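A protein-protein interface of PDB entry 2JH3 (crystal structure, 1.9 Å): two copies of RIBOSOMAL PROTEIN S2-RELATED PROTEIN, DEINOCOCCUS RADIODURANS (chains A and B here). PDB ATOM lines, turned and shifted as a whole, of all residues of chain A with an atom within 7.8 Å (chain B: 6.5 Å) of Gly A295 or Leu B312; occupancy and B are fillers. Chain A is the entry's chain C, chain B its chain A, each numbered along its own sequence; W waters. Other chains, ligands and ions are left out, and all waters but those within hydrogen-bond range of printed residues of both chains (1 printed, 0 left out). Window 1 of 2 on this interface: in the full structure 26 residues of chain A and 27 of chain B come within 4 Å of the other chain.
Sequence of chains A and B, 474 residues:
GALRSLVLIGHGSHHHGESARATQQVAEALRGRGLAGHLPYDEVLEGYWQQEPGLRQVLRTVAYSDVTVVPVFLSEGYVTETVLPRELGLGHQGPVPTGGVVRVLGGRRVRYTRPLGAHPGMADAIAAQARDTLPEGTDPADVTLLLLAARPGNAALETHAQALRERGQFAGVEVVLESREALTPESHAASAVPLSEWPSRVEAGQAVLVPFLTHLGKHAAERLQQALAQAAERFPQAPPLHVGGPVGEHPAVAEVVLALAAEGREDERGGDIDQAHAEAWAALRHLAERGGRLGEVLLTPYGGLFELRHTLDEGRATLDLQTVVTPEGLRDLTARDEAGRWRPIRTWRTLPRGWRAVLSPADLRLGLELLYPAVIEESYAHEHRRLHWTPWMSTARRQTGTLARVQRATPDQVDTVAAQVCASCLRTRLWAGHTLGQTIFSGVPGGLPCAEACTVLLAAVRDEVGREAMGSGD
Of the 25 printed residues of chain A, 9 touch a printed residue of chain B.
Hydrophobic or aromatic side chains of chain A that line the printed part of chain B: Leu A426, Val A444 and Pro A445.
Of the 12 printed residues of chain B, 10 touch a printed residue of chain A.
Hydrophobic or aromatic side chains of chain B that line the printed part of chain A: His B310 and Leu B312.
Along chain B the printed residues that touch a printed residue of chain A span positions 296 to 353.
Among the printed residues, 20 pairs touch across the chains.
Of the printed residues of chain B, Pro A445 touches Thr B311, Leu B312 and Glu B314.
Printed residues of chain A within 4 Å of Glu B296: Arg A349.
Leu B312 touches just these residues of chain A: Gly A295, Leu A426, Val A444, Pro A445 and Gly A446.
Printed residues of chain A within 4 Å of Glu B338: Arg A349.
The backbone NH (N) of Thr B311 is in hydrogen-bond range of the backbone carbonyl oxygen (O) of Glu B296, 2.8 Å away.
ND1 of His B310 sits at hydrogen-bond distance from N of Leu B312 (3.0 Å).
O of Leu B351 lies within hydrogen-bond range of NE2 of His B310, at 3.2 Å.
The side-chain carboxylate (OE2) of Glu B338 lies within salt-bridge range of the guanidinium group (NE) of Arg B353, at 3.0 Å.
The backbone NH (N) of Gly A295 sits at hydrogen-bond distance from the backbone carbonyl oxygen (O) of Pro A445 (2.9 Å).
The backbone NH (N) of Leu A426 sits at hydrogen-bond distance from the backbone carbonyl oxygen (O) of Thr A347 (2.9 Å).
Among the printed residues, pairs that only touch across the chains: Gly A295 with Leu B312 (3.7 Å), Arg A349 with His B310 (3.5 Å), Leu A426 with Leu B312 (3.8 Å), Gly A443 with Gly B315 (3.8 Å), Val A444 with Leu B312 (3.5 Å), Val A444 with Glu B314 (3.4 Å), Val A444 with Gly B315 (3.8 Å), Val A444 with Arg B316 (3.5 Å), Pro A445 with Thr B311 (3.9 Å), Pro A445 with Leu B312 (3.7 Å) and Pro A445 with Glu B314 (3.3 Å).
Positions printed for both chains: 296, 309, 310, 311 and 351.
Of the 20 pairs that touch across the chains among the printed residues, none has its exchanged pair printed and touching as well.
Water W1 lies within hydrogen-bond range of O of Cys A425, NH2 of Arg A349 and NH2 of Arg B353.
OE2 of Glu B296 lies within salt-bridge range of NH1 of Arg A349.
The backbone carbonyl oxygen (O) of Leu B312 sits at hydrogen-bond distance from the backbone NH (N) of Gly A446, 3.0 Å away.
OE1 of Glu B314 is in salt-bridge range of NE of Arg A293 (3.5 Å).
The side-chain carboxylate of Glu B338 lies within salt-bridge range of the guanidinium group of Arg A349.
The backbone carbonyl oxygen (O) of Leu B351 sits at hydrogen-bond distance from the guanidinium group (NH1) of Arg A349, at 2.8 Å.
The guanidinium group (NH2) of Arg B353 lies within hydrogen-bond range of the backbone carbonyl oxygen (O) of Cys A425, 3.2 Å away.
The backbone carbonyl oxygen (O) of Leu A426 sits at hydrogen-bond distance from the guanidinium group (NH1) of Arg B353, at 2.8 Å.
NH1 of Arg B353 is in hydrogen-bond range of O of Gly A446, 3.0 Å away.
The backbone carbonyl oxygen of Gly A443 sits close to the backbone carbonyl oxygen of Glu B314, at 3.1 Å.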
ATOM      1  N   GLY A 292     -21.234   4.858   3.643  1.00  0.00           N
ATOM      2  CA  GLY A 292     -22.074   5.675   2.859  1.00  0.00           C
ATOM      3  C   GLY A 292     -21.390   6.005   1.544  1.00  0.00           C
ATOM      4  O   GLY A 292     -20.212   5.652   1.305  1.00  0.00           O
ATOM      5  N   ARG A 293     -22.137   6.686   0.698  1.00  0.00           N
ATOM      6  CA  ARG A 293     -21.654   7.000  -0.626  1.00  0.00           C
ATOM      7  C   ARG A 293     -21.795   8.473  -0.884  1.00  0.00           C
ATOM      8  O   ARG A 293     -22.808   9.073  -0.498  1.00  0.00           O
ATOM      9  CB  ARG A 293     -22.441   6.237  -1.676  1.00  0.00           C
ATOM     10  CG  ARG A 293     -22.363   4.724  -1.531  1.00  0.00           C
ATOM     11  CD  ARG A 293     -23.492   4.033  -2.284  1.00  0.00           C
ATOM     12  NE  ARG A 293     -23.398   2.591  -2.027  1.00  0.00           N
ATOM     13  CZ  ARG A 293     -22.699   1.757  -2.735  1.00  0.00           C
ATOM     14  NH1 ARG A 293     -22.118   2.183  -3.789  1.00  0.00           N
ATOM     15  NH2 ARG A 293     -22.630   0.449  -2.393  1.00  0.00           N
ATOM     16  N   LEU A 294     -20.821   9.053  -1.546  1.00  0.00           N
ATOM     17  CA  LEU A 294     -20.790  10.494  -1.834  1.00  0.00           C
ATOM     18  C   LEU A 294     -20.260  10.662  -3.229  1.00  0.00           C
ATOM     19  O   LEU A 294     -19.139  10.294  -3.540  1.00  0.00           O
ATOM     20  CB  LEU A 294     -19.848  11.295  -0.917  1.00  0.00           C
ATOM     21  CG  LEU A 294     -19.865  11.125   0.577  1.00  0.00           C
ATOM     22  CD1 LEU A 294     -18.813  12.057   1.181  1.00  0.00           C
ATOM     23  CD2 LEU A 294     -21.255  11.390   1.196  1.00  0.00           C
ATOM     24  N   GLY A 295     -21.080  11.208  -4.109  1.00  0.00           N
ATOM     25  CA  GLY A 295     -20.693  11.256  -5.509  1.00  0.00           C
ATOM     26  C   GLY A 295     -20.421   9.892  -6.111  1.00  0.00           C
ATOM     27  O   GLY A 295     -21.267   8.998  -6.058  1.00  0.00           O
ATOM     28  N   GLU A 296     -19.242   9.742  -6.704  1.00  0.00           N
ATOM     29  CA  GLU A 296     -18.736   8.470  -7.232  1.00  0.00           C
ATOM     30  C   GLU A 296     -17.816   7.773  -6.260  1.00  0.00           C
ATOM     31  O   GLU A 296     -17.107   6.857  -6.620  1.00  0.00           O
ATOM     32  CB  GLU A 296     -17.992   8.700  -8.530  1.00  0.00           C
ATOM     33  CG  GLU A 296     -18.822   9.286  -9.589  1.00  0.00           C
ATOM     34  CD  GLU A 296     -18.018   9.481 -10.964  1.00  0.00           C
ATOM     35  OE1 GLU A 296     -17.284  10.470 -11.043  1.00  0.00           O
ATOM     36  OE2 GLU A 296     -18.149   8.671 -11.898  1.00  0.00           O
ATOM     37  N   VAL A 297     -17.897   8.135  -4.987  1.00  0.00           N
ATOM     38  CA  VAL A 297     -16.998   7.605  -3.964  1.00  0.00           C
ATOM     39  C   VAL A 297     -17.803   6.831  -2.880  1.00  0.00           C
ATOM     40  O   VAL A 297     -18.842   7.295  -2.332  1.00  0.00           O
ATOM     41  CB  VAL A 297     -16.153   8.759  -3.361  1.00  0.00           C
ATOM     42  CG1 VAL A 297     -15.508   8.391  -2.072  1.00  0.00           C
ATOM     43  CG2 VAL A 297     -15.153   9.226  -4.340  1.00  0.00           C
ATOM     44  N   LEU A 298     -17.296   5.660  -2.632  1.00  0.00           N
ATOM     45  CA  LEU A 298     -17.710   4.772  -1.560  1.00  0.00           C
ATOM     46  C   LEU A 298     -16.764   4.931  -0.331  1.00  0.00           C
ATOM     47  O   LEU A 298     -15.551   4.793  -0.441  1.00  0.00           O
ATOM     48  CB  LEU A 298     -17.673   3.316  -2.059  1.00  0.00           C
ATOM     49  CG  LEU A 298     -18.056   2.173  -1.090  1.00  0.00           C
ATOM     50  CD1 LEU A 298     -19.535   2.277  -0.748  1.00  0.00           C
ATOM     51  CD2 LEU A 298     -17.728   0.873  -1.707  1.00  0.00           C
ATOM     52  N   LEU A 299     -17.364   5.214   0.816  1.00  0.00           N
ATOM     53  CA  LEU A 299     -16.672   5.343   2.103  1.00  0.00           C
ATOM     54  C   LEU A 299     -17.023   4.183   3.015  1.00  0.00           C
ATOM     55  O   LEU A 299     -18.225   3.912   3.228  1.00  0.00           O
ATOM     56  CB  LEU A 299     -17.197   6.511   2.865  1.00  0.00           C
ATOM     57  CG  LEU A 299     -16.860   7.898   2.507  1.00  0.00           C
ATOM     58  CD1 LEU A 299     -17.685   8.317   1.359  1.00  0.00           C
ATOM     59  CD2 LEU A 299     -17.154   8.685   3.835  1.00  0.00           C
ATOM     60  N   ARG A 309     -12.941   4.406  -2.159  1.00  0.00           N
ATOM     61  CA  ARG A 309     -12.684   3.952  -3.500  1.00  0.00           C
ATOM     62  C   ARG A 309     -13.828   4.443  -4.381  1.00  0.00           C
ATOM     63  O   ARG A 309     -14.832   4.953  -3.900  1.00  0.00           O
ATOM     64  CB  ARG A 309     -12.607   2.400  -3.528  1.00  0.00           C
ATOM     65  CG  ARG A 309     -13.881   1.602  -3.121  1.00  0.00           C
ATOM     66  CD  ARG A 309     -13.741   0.237  -3.621  1.00  0.00           C
ATOM     67  NE  ARG A 309     -12.881  -0.495  -2.690  1.00  0.00           N
ATOM     68  CZ  ARG A 309     -12.395  -1.722  -2.849  1.00  0.00           C
ATOM     69  NH1 ARG A 309     -12.633  -2.484  -3.877  1.00  0.00           N
ATOM     70  NH2 ARG A 309     -11.618  -2.225  -1.866  1.00  0.00           N
ATOM     71  N   HIS A 310     -13.675   4.260  -5.677  1.00  0.00           N
ATOM     72  CA  HIS A 310     -14.759   4.589  -6.616  1.00  0.00           C
ATOM     73  C   HIS A 310     -15.891   3.584  -6.450  1.00  0.00           C
ATOM     74  O   HIS A 310     -15.627   2.409  -6.366  1.00  0.00           O
ATOM     75  CB  HIS A 310     -14.247   4.471  -8.083  1.00  0.00           C
ATOM     76  CG  HIS A 310     -15.055   5.216  -9.082  1.00  0.00           C
ATOM     77  ND1 HIS A 310     -16.330   4.814  -9.456  1.00  0.00           N
ATOM     78  CD2 HIS A 310     -14.753   6.284  -9.870  1.00  0.00           C
ATOM     79  CE1 HIS A 310     -16.792   5.671 -10.364  1.00  0.00           C
ATOM     80  NE2 HIS A 310     -15.845   6.539 -10.662  1.00  0.00           N
ATOM     81  N   THR A 311     -17.125   4.045  -6.507  1.00  0.00           N
ATOM     82  CA  THR A 311     -18.274   3.163  -6.371  1.00  0.00           C
ATOM     83  C   THR A 311     -18.250   2.084  -7.477  1.00  0.00           C
ATOM     84  O   THR A 311     -18.697   0.926  -7.271  1.00  0.00           O
ATOM     85  CB  THR A 311     -19.618   3.995  -6.395  1.00  0.00           C
ATOM     86  OG1 THR A 311     -19.595   4.963  -7.460  1.00  0.00           O
ATOM     87  CG2 THR A 311     -19.785   4.695  -5.140  1.00  0.00           C
ATOM     88  N   THR A 347     -16.391  17.718  -9.221  1.00  0.00           N
ATOM     89  CA  THR A 347     -17.692  17.032  -9.168  1.00  0.00           C
ATOM     90  C   THR A 347     -18.111  16.542 -10.512  1.00  0.00           C
ATOM     91  O   THR A 347     -19.227  16.048 -10.649  1.00  0.00           O
ATOM     92  CB  THR A 347     -18.833  17.967  -8.601  1.00  0.00           C
ATOM     93  OG1 THR A 347     -18.812  19.254  -9.236  1.00  0.00           O
ATOM     94  CG2 THR A 347     -18.613  18.249  -7.212  1.00  0.00           C
ATOM     95  N   ARG A 349     -18.564  13.937 -13.427  1.00  0.00           N
ATOM     96  CA  ARG A 349     -18.784  12.498 -13.402  1.00  0.00           C
ATOM     97  C   ARG A 349     -17.674  11.738 -14.232  1.00  0.00           C
ATOM     98  O   ARG A 349     -17.969  10.979 -15.166  1.00  0.00           O
ATOM     99  CB  ARG A 349     -20.204  12.179 -13.913  1.00  0.00           C
ATOM    100  CG  ARG A 349     -20.806  10.903 -13.307  1.00  0.00           C
ATOM    101  CD  ARG A 349     -21.799  10.247 -14.337  1.00  0.00           C
ATOM    102  NE  ARG A 349     -22.914  11.163 -14.493  1.00  0.00           N
ATOM    103  CZ  ARG A 349     -24.062  10.823 -15.074  1.00  0.00           C
ATOM    104  NH1 ARG A 349     -24.241   9.603 -15.499  1.00  0.00           N
ATOM    105  NH2 ARG A 349     -25.035  11.696 -15.165  1.00  0.00           N
ATOM    106  N   LEU A 351     -14.530  10.826 -12.388  1.00  0.00           N
ATOM    107  CA  LEU A 351     -13.568  10.288 -11.392  1.00  0.00           C
ATOM    108  C   LEU A 351     -13.002   9.031 -11.977  1.00  0.00           C
ATOM    109  O   LEU A 351     -13.781   8.238 -12.416  1.00  0.00           O
ATOM    110  CB  LEU A 351     -14.229  10.041 -10.040  1.00  0.00           C
ATOM    111  CG  LEU A 351     -13.372   9.871  -8.788  1.00  0.00           C
ATOM    112  CD1 LEU A 351     -12.592  11.143  -8.426  1.00  0.00           C
ATOM    113  CD2 LEU A 351     -14.307   9.502  -7.641  1.00  0.00           C
ATOM    114  N   TYR A 372     -13.131  16.286  -3.133  1.00  0.00           N
ATOM    115  CA  TYR A 372     -14.360  16.992  -3.526  1.00  0.00           C
ATOM    116  C   TYR A 372     -14.474  18.349  -2.837  1.00  0.00           C
ATOM    117  O   TYR A 372     -15.333  18.568  -2.024  1.00  0.00           O
ATOM    118  CB  TYR A 372     -15.611  16.130  -3.157  1.00  0.00           C
ATOM    119  CG  TYR A 372     -15.976  14.974  -4.073  1.00  0.00           C
ATOM    120  CD1 TYR A 372     -16.142  15.193  -5.411  1.00  0.00           C
ATOM    121  CD2 TYR A 372     -16.284  13.693  -3.581  1.00  0.00           C
ATOM    122  CE1 TYR A 372     -16.523  14.175  -6.274  1.00  0.00           C
ATOM    123  CE2 TYR A 372     -16.682  12.644  -4.462  1.00  0.00           C
ATOM    124  CZ  TYR A 372     -16.825  12.918  -5.816  1.00  0.00           C
ATOM    125  OH  TYR A 372     -17.202  11.994  -6.787  1.00  0.00           O
ATOM    126  N   VAL A 375     -17.944  20.488  -1.338  1.00  0.00           N
ATOM    127  CA  VAL A 375     -19.146  19.663  -1.433  1.00  0.00           C
ATOM    128  C   VAL A 375     -19.735  19.375  -0.037  1.00  0.00           C
ATOM    129  O   VAL A 375     -20.916  19.436   0.136  1.00  0.00           O
ATOM    130  CB  VAL A 375     -18.820  18.335  -2.166  1.00  0.00           C
ATOM    131  CG1 VAL A 375     -19.960  17.340  -2.134  1.00  0.00           C
ATOM    132  CG2 VAL A 375     -18.469  18.596  -3.599  1.00  0.00           C
ATOM    133  N   CYS A 425     -21.665  17.051 -14.962  1.00  0.00           N
ATOM    134  CA  CYS A 425     -21.434  17.345 -13.566  1.00  0.00           C
ATOM    135  C   CYS A 425     -22.441  16.647 -12.640  1.00  0.00           C
ATOM    136  O   CYS A 425     -23.564  16.467 -12.983  1.00  0.00           O
ATOM    137  CB  CYS A 425     -21.528  18.874 -13.379  1.00  0.00           C
ATOM    138  SG  CYS A 425     -20.998  19.625 -11.761  1.00  0.00           S
ATOM    139  N   LEU A 426     -22.020  16.296 -11.433  1.00  0.00           N
ATOM    140  CA  LEU A 426     -22.886  15.710 -10.437  1.00  0.00           C
ATOM    141  C   LEU A 426     -23.804  16.719  -9.781  1.00  0.00           C
ATOM    142  O   LEU A 426     -24.845  16.351  -9.290  1.00  0.00           O
ATOM    143  CB  LEU A 426     -22.025  15.174  -9.314  1.00  0.00           C
ATOM    144  CG  LEU A 426     -21.643  13.704  -9.259  1.00  0.00           C
ATOM    145  CD1 LEU A 426     -21.976  12.823 -10.373  1.00  0.00           C
ATOM    146  CD2 LEU A 426     -20.297  13.567  -8.748  1.00  0.00           C
ATOM    147  N   ILE A 440     -26.508  14.256  -0.409  1.00  0.00           N
ATOM    148  CA  ILE A 440     -25.657  13.212   0.191  1.00  0.00           C
ATOM    149  C   ILE A 440     -25.891  12.954   1.691  1.00  0.00           C
ATOM    150  O   ILE A 440     -25.608  11.859   2.211  1.00  0.00           O
ATOM    151  CB  ILE A 440     -24.113  13.508  -0.052  1.00  0.00           C
ATOM    152  CG1 ILE A 440     -23.738  14.967   0.402  1.00  0.00           C
ATOM    153  CG2 ILE A 440     -23.761  13.394  -1.539  1.00  0.00           C
ATOM    154  CD1 ILE A 440     -22.233  15.197   0.683  1.00  0.00           C
ATOM    155  N   GLY A 443     -29.257  10.665   2.090  1.00  0.00           N
ATOM    156  CA  GLY A 443     -29.213   9.345   1.464  1.00  0.00           C
ATOM    157  C   GLY A 443     -28.866   9.224   0.000  1.00  0.00           C
ATOM    158  O   GLY A 443     -28.830   8.132  -0.505  1.00  0.00           O
ATOM    159  N   VAL A 444     -28.669  10.346  -0.693  1.00  0.00           N
ATOM    160  CA  VAL A 444     -28.686  10.362  -2.152  1.00  0.00           C
ATOM    161  C   VAL A 444     -27.253  10.670  -2.615  1.00  0.00           C
ATOM    162  O   VAL A 444     -26.836  11.837  -2.525  1.00  0.00           O
ATOM    163  CB  VAL A 444     -29.719  11.375  -2.732  1.00  0.00           C
ATOM    164  CG1 VAL A 444     -29.689  11.413  -4.223  1.00  0.00           C
ATOM    165  CG2 VAL A 444     -31.119  10.986  -2.385  1.00  0.00           C
ATOM    166  N   PRO A 445     -26.524   9.654  -3.112  1.00  0.00           N
ATOM    167  CA  PRO A 445     -25.123   9.903  -3.497  1.00  0.00           C
ATOM    168  C   PRO A 445     -24.904  11.013  -4.505  1.00  0.00           C
ATOM    169  O   PRO A 445     -23.908  11.743  -4.411  1.00  0.00           O
ATOM    170  CB  PRO A 445     -24.677   8.573  -4.098  1.00  0.00           C
ATOM    171  CG  PRO A 445     -25.588   7.566  -3.483  1.00  0.00           C
ATOM    172  CD  PRO A 445     -26.900   8.247  -3.315  1.00  0.00           C
ATOM    173  N   GLY A 446     -25.805  11.136  -5.483  1.00  0.00           N
ATOM    174  CA  GLY A 446     -25.695  12.152  -6.519  1.00  0.00           C
ATOM    175  C   GLY A 446     -26.373  13.476  -6.289  1.00  0.00           C
ATOM    176  O   GLY A 446     -26.592  14.207  -7.243  1.00  0.00           O
ATOM    177  N   GLY A 447     -26.722  13.745  -5.030  1.00  0.00           N
ATOM    178  CA  GLY A 447     -27.442  14.931  -4.612  1.00  0.00           C
ATOM    179  C   GLY A 447     -26.486  15.976  -4.042  1.00  0.00           C
ATOM    180  O   GLY A 447     -26.130  15.939  -2.894  1.00  0.00           O
ATOM    181  N   LEU A 448     -26.018  16.832  -4.946  1.00  0.00           N
ATOM    182  CA  LEU A 448     -25.033  17.873  -4.624  1.00  0.00           C
ATOM    183  C   LEU A 448     -25.476  19.174  -5.240  1.00  0.00           C
ATOM    184  O   LEU A 448     -25.758  19.234  -6.463  1.00  0.00           O
ATOM    185  CB  LEU A 448     -23.682  17.549  -5.249  1.00  0.00           C
ATOM    186  CG  LEU A 448     -22.831  16.392  -4.760  1.00  0.00           C
ATOM    187  CD1 LEU A 448     -23.326  15.028  -5.069  1.00  0.00           C
ATOM    188  CD2 LEU A 448     -21.437  16.544  -5.404  1.00  0.00           C
ATOM    189  N   GLU B 296     -24.101   1.628 -14.024  1.00  0.00           N
ATOM    190  CA  GLU B 296     -24.659   2.745 -13.312  1.00  0.00           C
ATOM    191  C   GLU B 296     -26.105   2.501 -12.846  1.00  0.00           C
ATOM    192  O   GLU B 296     -26.793   3.470 -12.440  1.00  0.00           O
ATOM    193  CB  GLU B 296     -24.685   3.964 -14.218  1.00  0.00           C
ATOM    194  CG  GLU B 296     -23.311   4.623 -14.534  1.00  0.00           C
ATOM    195  CD  GLU B 296     -23.477   6.010 -15.298  1.00  0.00           C
ATOM    196  OE1 GLU B 296     -23.753   5.985 -16.523  1.00  0.00           O
ATOM    197  OE2 GLU B 296     -23.226   7.089 -14.686  1.00  0.00           O
ATOM    198  N   ARG B 309     -33.031   1.755 -10.954  1.00  0.00           N
ATOM    199  CA  ARG B 309     -32.838   3.214 -10.948  1.00  0.00           C
ATOM    200  C   ARG B 309     -31.352   3.462 -11.114  1.00  0.00           C
ATOM    201  O   ARG B 309     -30.541   2.541 -11.048  1.00  0.00           O
ATOM    202  CB  ARG B 309     -33.344   3.879  -9.647  1.00  0.00           C
ATOM    203  CG  ARG B 309     -32.558   3.528  -8.449  1.00  0.00           C
ATOM    204  CD  ARG B 309     -33.027   4.253  -7.236  1.00  0.00           C
ATOM    205  NE  ARG B 309     -34.453   4.045  -6.853  1.00  0.00           N
ATOM    206  CZ  ARG B 309     -35.057   4.775  -5.931  1.00  0.00           C
ATOM    207  NH1 ARG B 309     -34.440   5.742  -5.274  1.00  0.00           N
ATOM    208  NH2 ARG B 309     -36.281   4.532  -5.610  1.00  0.00           N
ATOM    209  N   HIS B 310     -30.977   4.728 -11.308  1.00  0.00           N
ATOM    210  CA  HIS B 310     -29.557   5.067 -11.425  1.00  0.00           C
ATOM    211  C   HIS B 310     -28.943   4.906 -10.030  1.00  0.00           C
ATOM    212  O   HIS B 310     -29.525   5.311  -9.042  1.00  0.00           O
ATOM    213  CB  HIS B 310     -29.428   6.487 -11.929  1.00  0.00           C
ATOM    214  CG  HIS B 310     -28.096   6.838 -12.469  1.00  0.00           C
ATOM    215  ND1 HIS B 310     -26.977   6.928 -11.685  1.00  0.00           N
ATOM    216  CD2 HIS B 310     -27.726   7.247 -13.693  1.00  0.00           C
ATOM    217  CE1 HIS B 310     -25.965   7.346 -12.427  1.00  0.00           C
ATOM    218  NE2 HIS B 310     -26.392   7.544 -13.642  1.00  0.00           N
ATOM    219  N   THR B 311     -27.725   4.366  -9.932  1.00  0.00           N
ATOM    220  CA  THR B 311     -27.052   4.332  -8.673  1.00  0.00           C
ATOM    221  C   THR B 311     -26.870   5.691  -7.956  1.00  0.00           C
ATOM    222  O   THR B 311     -26.901   5.738  -6.719  1.00  0.00           O
ATOM    223  CB  THR B 311     -25.716   3.638  -8.813  1.00  0.00           C
ATOM    224  OG1 THR B 311     -25.018   4.212  -9.889  1.00  0.00           O
ATOM    225  CG2 THR B 311     -25.872   2.173  -9.099  1.00  0.00           C
ATOM    226  N   LEU B 312     -26.728   6.800  -8.674  1.00  0.00           N
ATOM    227  CA  LEU B 312     -26.668   8.115  -8.080  1.00  0.00           C
ATOM    228  C   LEU B 312     -27.991   8.527  -7.386  1.00  0.00           C
ATOM    229  O   LEU B 312     -28.013   9.443  -6.580  1.00  0.00           O
ATOM    230  CB  LEU B 312     -26.282   9.215  -9.135  1.00  0.00           C
ATOM    231  CG  LEU B 312     -24.816   9.202  -9.683  1.00  0.00           C
ATOM    232  CD1 LEU B 312     -24.690  10.208 -10.823  1.00  0.00           C
ATOM    233  CD2 LEU B 312     -23.861   9.495  -8.606  1.00  0.00           C
ATOM    234  N   ASP B 313     -29.095   7.918  -7.819  1.00  0.00           N
ATOM    235  CA  ASP B 313     -30.411   8.134  -7.257  1.00  0.00           C
ATOM    236  C   ASP B 313     -30.745   7.125  -6.141  1.00  0.00           C
ATOM    237  O   ASP B 313     -31.884   7.105  -5.731  1.00  0.00           O
ATOM    238  CB  ASP B 313     -31.490   8.016  -8.401  1.00  0.00           C
ATOM    239  CG  ASP B 313     -31.517   9.250  -9.310  1.00  0.00           C
ATOM    240  OD1 ASP B 313     -31.111  10.372  -8.853  1.00  0.00           O
ATOM    241  OD2 ASP B 313     -31.926   9.088 -10.484  1.00  0.00           O
ATOM    242  N   GLU B 314     -29.805   6.245  -5.693  1.00  0.00           N
ATOM    243  CA  GLU B 314     -30.036   5.461  -4.498  1.00  0.00           C
ATOM    244  C   GLU B 314     -30.577   6.316  -3.360  1.00  0.00           C
ATOM    245  O   GLU B 314     -30.137   7.421  -3.213  1.00  0.00           O
ATOM    246  CB  GLU B 314     -28.762   4.713  -4.054  1.00  0.00           C
ATOM    247  CG  GLU B 314     -29.099   3.700  -3.015  1.00  0.00           C
ATOM    248  CD  GLU B 314     -27.948   2.944  -2.437  1.00  0.00           C
ATOM    249  OE1 GLU B 314     -26.782   3.081  -2.904  1.00  0.00           O
ATOM    250  OE2 GLU B 314     -28.281   2.121  -1.553  1.00  0.00           O
ATOM    251  N   GLY B 315     -31.606   5.865  -2.611  1.00  0.00           N
ATOM    252  CA  GLY B 315     -32.134   6.644  -1.488  1.00  0.00           C
ATOM    253  C   GLY B 315     -33.103   7.788  -1.853  1.00  0.00           C
ATOM    254  O   GLY B 315     -33.768   8.413  -1.012  1.00  0.00           O
ATOM    255  N   ARG B 316     -33.228   8.071  -3.125  1.00  0.00           N
ATOM    256  CA  ARG B 316     -33.976   9.224  -3.518  1.00  0.00           C
ATOM    257  C   ARG B 316     -35.478   8.911  -3.406  1.00  0.00           C
ATOM    258  O   ARG B 316     -35.936   7.853  -3.805  1.00  0.00           O
ATOM    259  CB  ARG B 316     -33.631   9.611  -4.962  1.00  0.00           C
ATOM    260  CG  ARG B 316     -34.082  10.936  -5.331  1.00  0.00           C
ATOM    261  CD  ARG B 316     -33.380  11.373  -6.588  1.00  0.00           C
ATOM    262  NE  ARG B 316     -34.065  12.474  -7.186  1.00  0.00           N
ATOM    263  CZ  ARG B 316     -33.854  12.963  -8.390  1.00  0.00           C
ATOM    264  NH1 ARG B 316     -32.947  12.506  -9.249  1.00  0.00           N
ATOM    265  NH2 ARG B 316     -34.585  13.971  -8.744  1.00  0.00           N
ATOM    266  N   GLU B 338     -28.099  13.687 -19.990  1.00  0.00           N
ATOM    267  CA  GLU B 338     -28.721  14.824 -19.322  1.00  0.00           C
ATOM    268  C   GLU B 338     -28.682  16.134 -20.119  1.00  0.00           C
ATOM    269  O   GLU B 338     -29.421  17.062 -19.784  1.00  0.00           O
ATOM    270  CB  GLU B 338     -28.180  14.986 -17.874  1.00  0.00           C
ATOM    271  CG  GLU B 338     -28.680  13.828 -16.960  1.00  0.00           C
ATOM    272  CD  GLU B 338     -28.050  13.816 -15.591  1.00  0.00           C
ATOM    273  OE1 GLU B 338     -27.336  14.774 -15.252  1.00  0.00           O
ATOM    274  OE2 GLU B 338     -28.292  12.887 -14.816  1.00  0.00           O
ATOM    275  N   LEU B 351     -25.473   7.802 -18.236  1.00  0.00           N
ATOM    276  CA  LEU B 351     -26.854   7.411 -18.024  1.00  0.00           C
ATOM    277  C   LEU B 351     -27.454   8.572 -17.278  1.00  0.00           C
ATOM    278  O   LEU B 351     -26.852   9.084 -16.386  1.00  0.00           O
ATOM    279  CB  LEU B 351     -26.950   6.147 -17.185  1.00  0.00           C
ATOM    280  CG  LEU B 351     -28.240   5.368 -17.102  1.00  0.00           C
ATOM    281  CD1 LEU B 351     -28.486   4.825 -18.411  1.00  0.00           C
ATOM    282  CD2 LEU B 351     -28.103   4.281 -16.063  1.00  0.00           C
ATOM    283  N   ARG B 353     -30.047  10.586 -14.714  1.00  0.00           N
ATOM    284  CA  ARG B 353     -30.729  10.468 -13.474  1.00  0.00           C
ATOM    285  C   ARG B 353     -32.219  10.779 -13.656  1.00  0.00           C
ATOM    286  O   ARG B 353     -32.664  11.192 -14.704  1.00  0.00           O
ATOM    287  CB  ARG B 353     -30.106  11.368 -12.402  1.00  0.00           C
ATOM    288  CG  ARG B 353     -28.766  10.917 -11.938  1.00  0.00           C
ATOM    289  CD  ARG B 353     -28.075  11.994 -11.090  1.00  0.00           C
ATOM    290  NE  ARG B 353     -27.502  13.036 -11.922  1.00  0.00           N
ATOM    291  CZ  ARG B 353     -26.778  14.090 -11.517  1.00  0.00           C
ATOM    292  NH1 ARG B 353     -26.562  14.295 -10.234  1.00  0.00           N
ATOM    293  NH2 ARG B 353     -26.244  14.899 -12.444  1.00  0.00           N
HETATM  294  O   HOH W   1     -23.529  14.136 -14.436  1.00  0.00           O
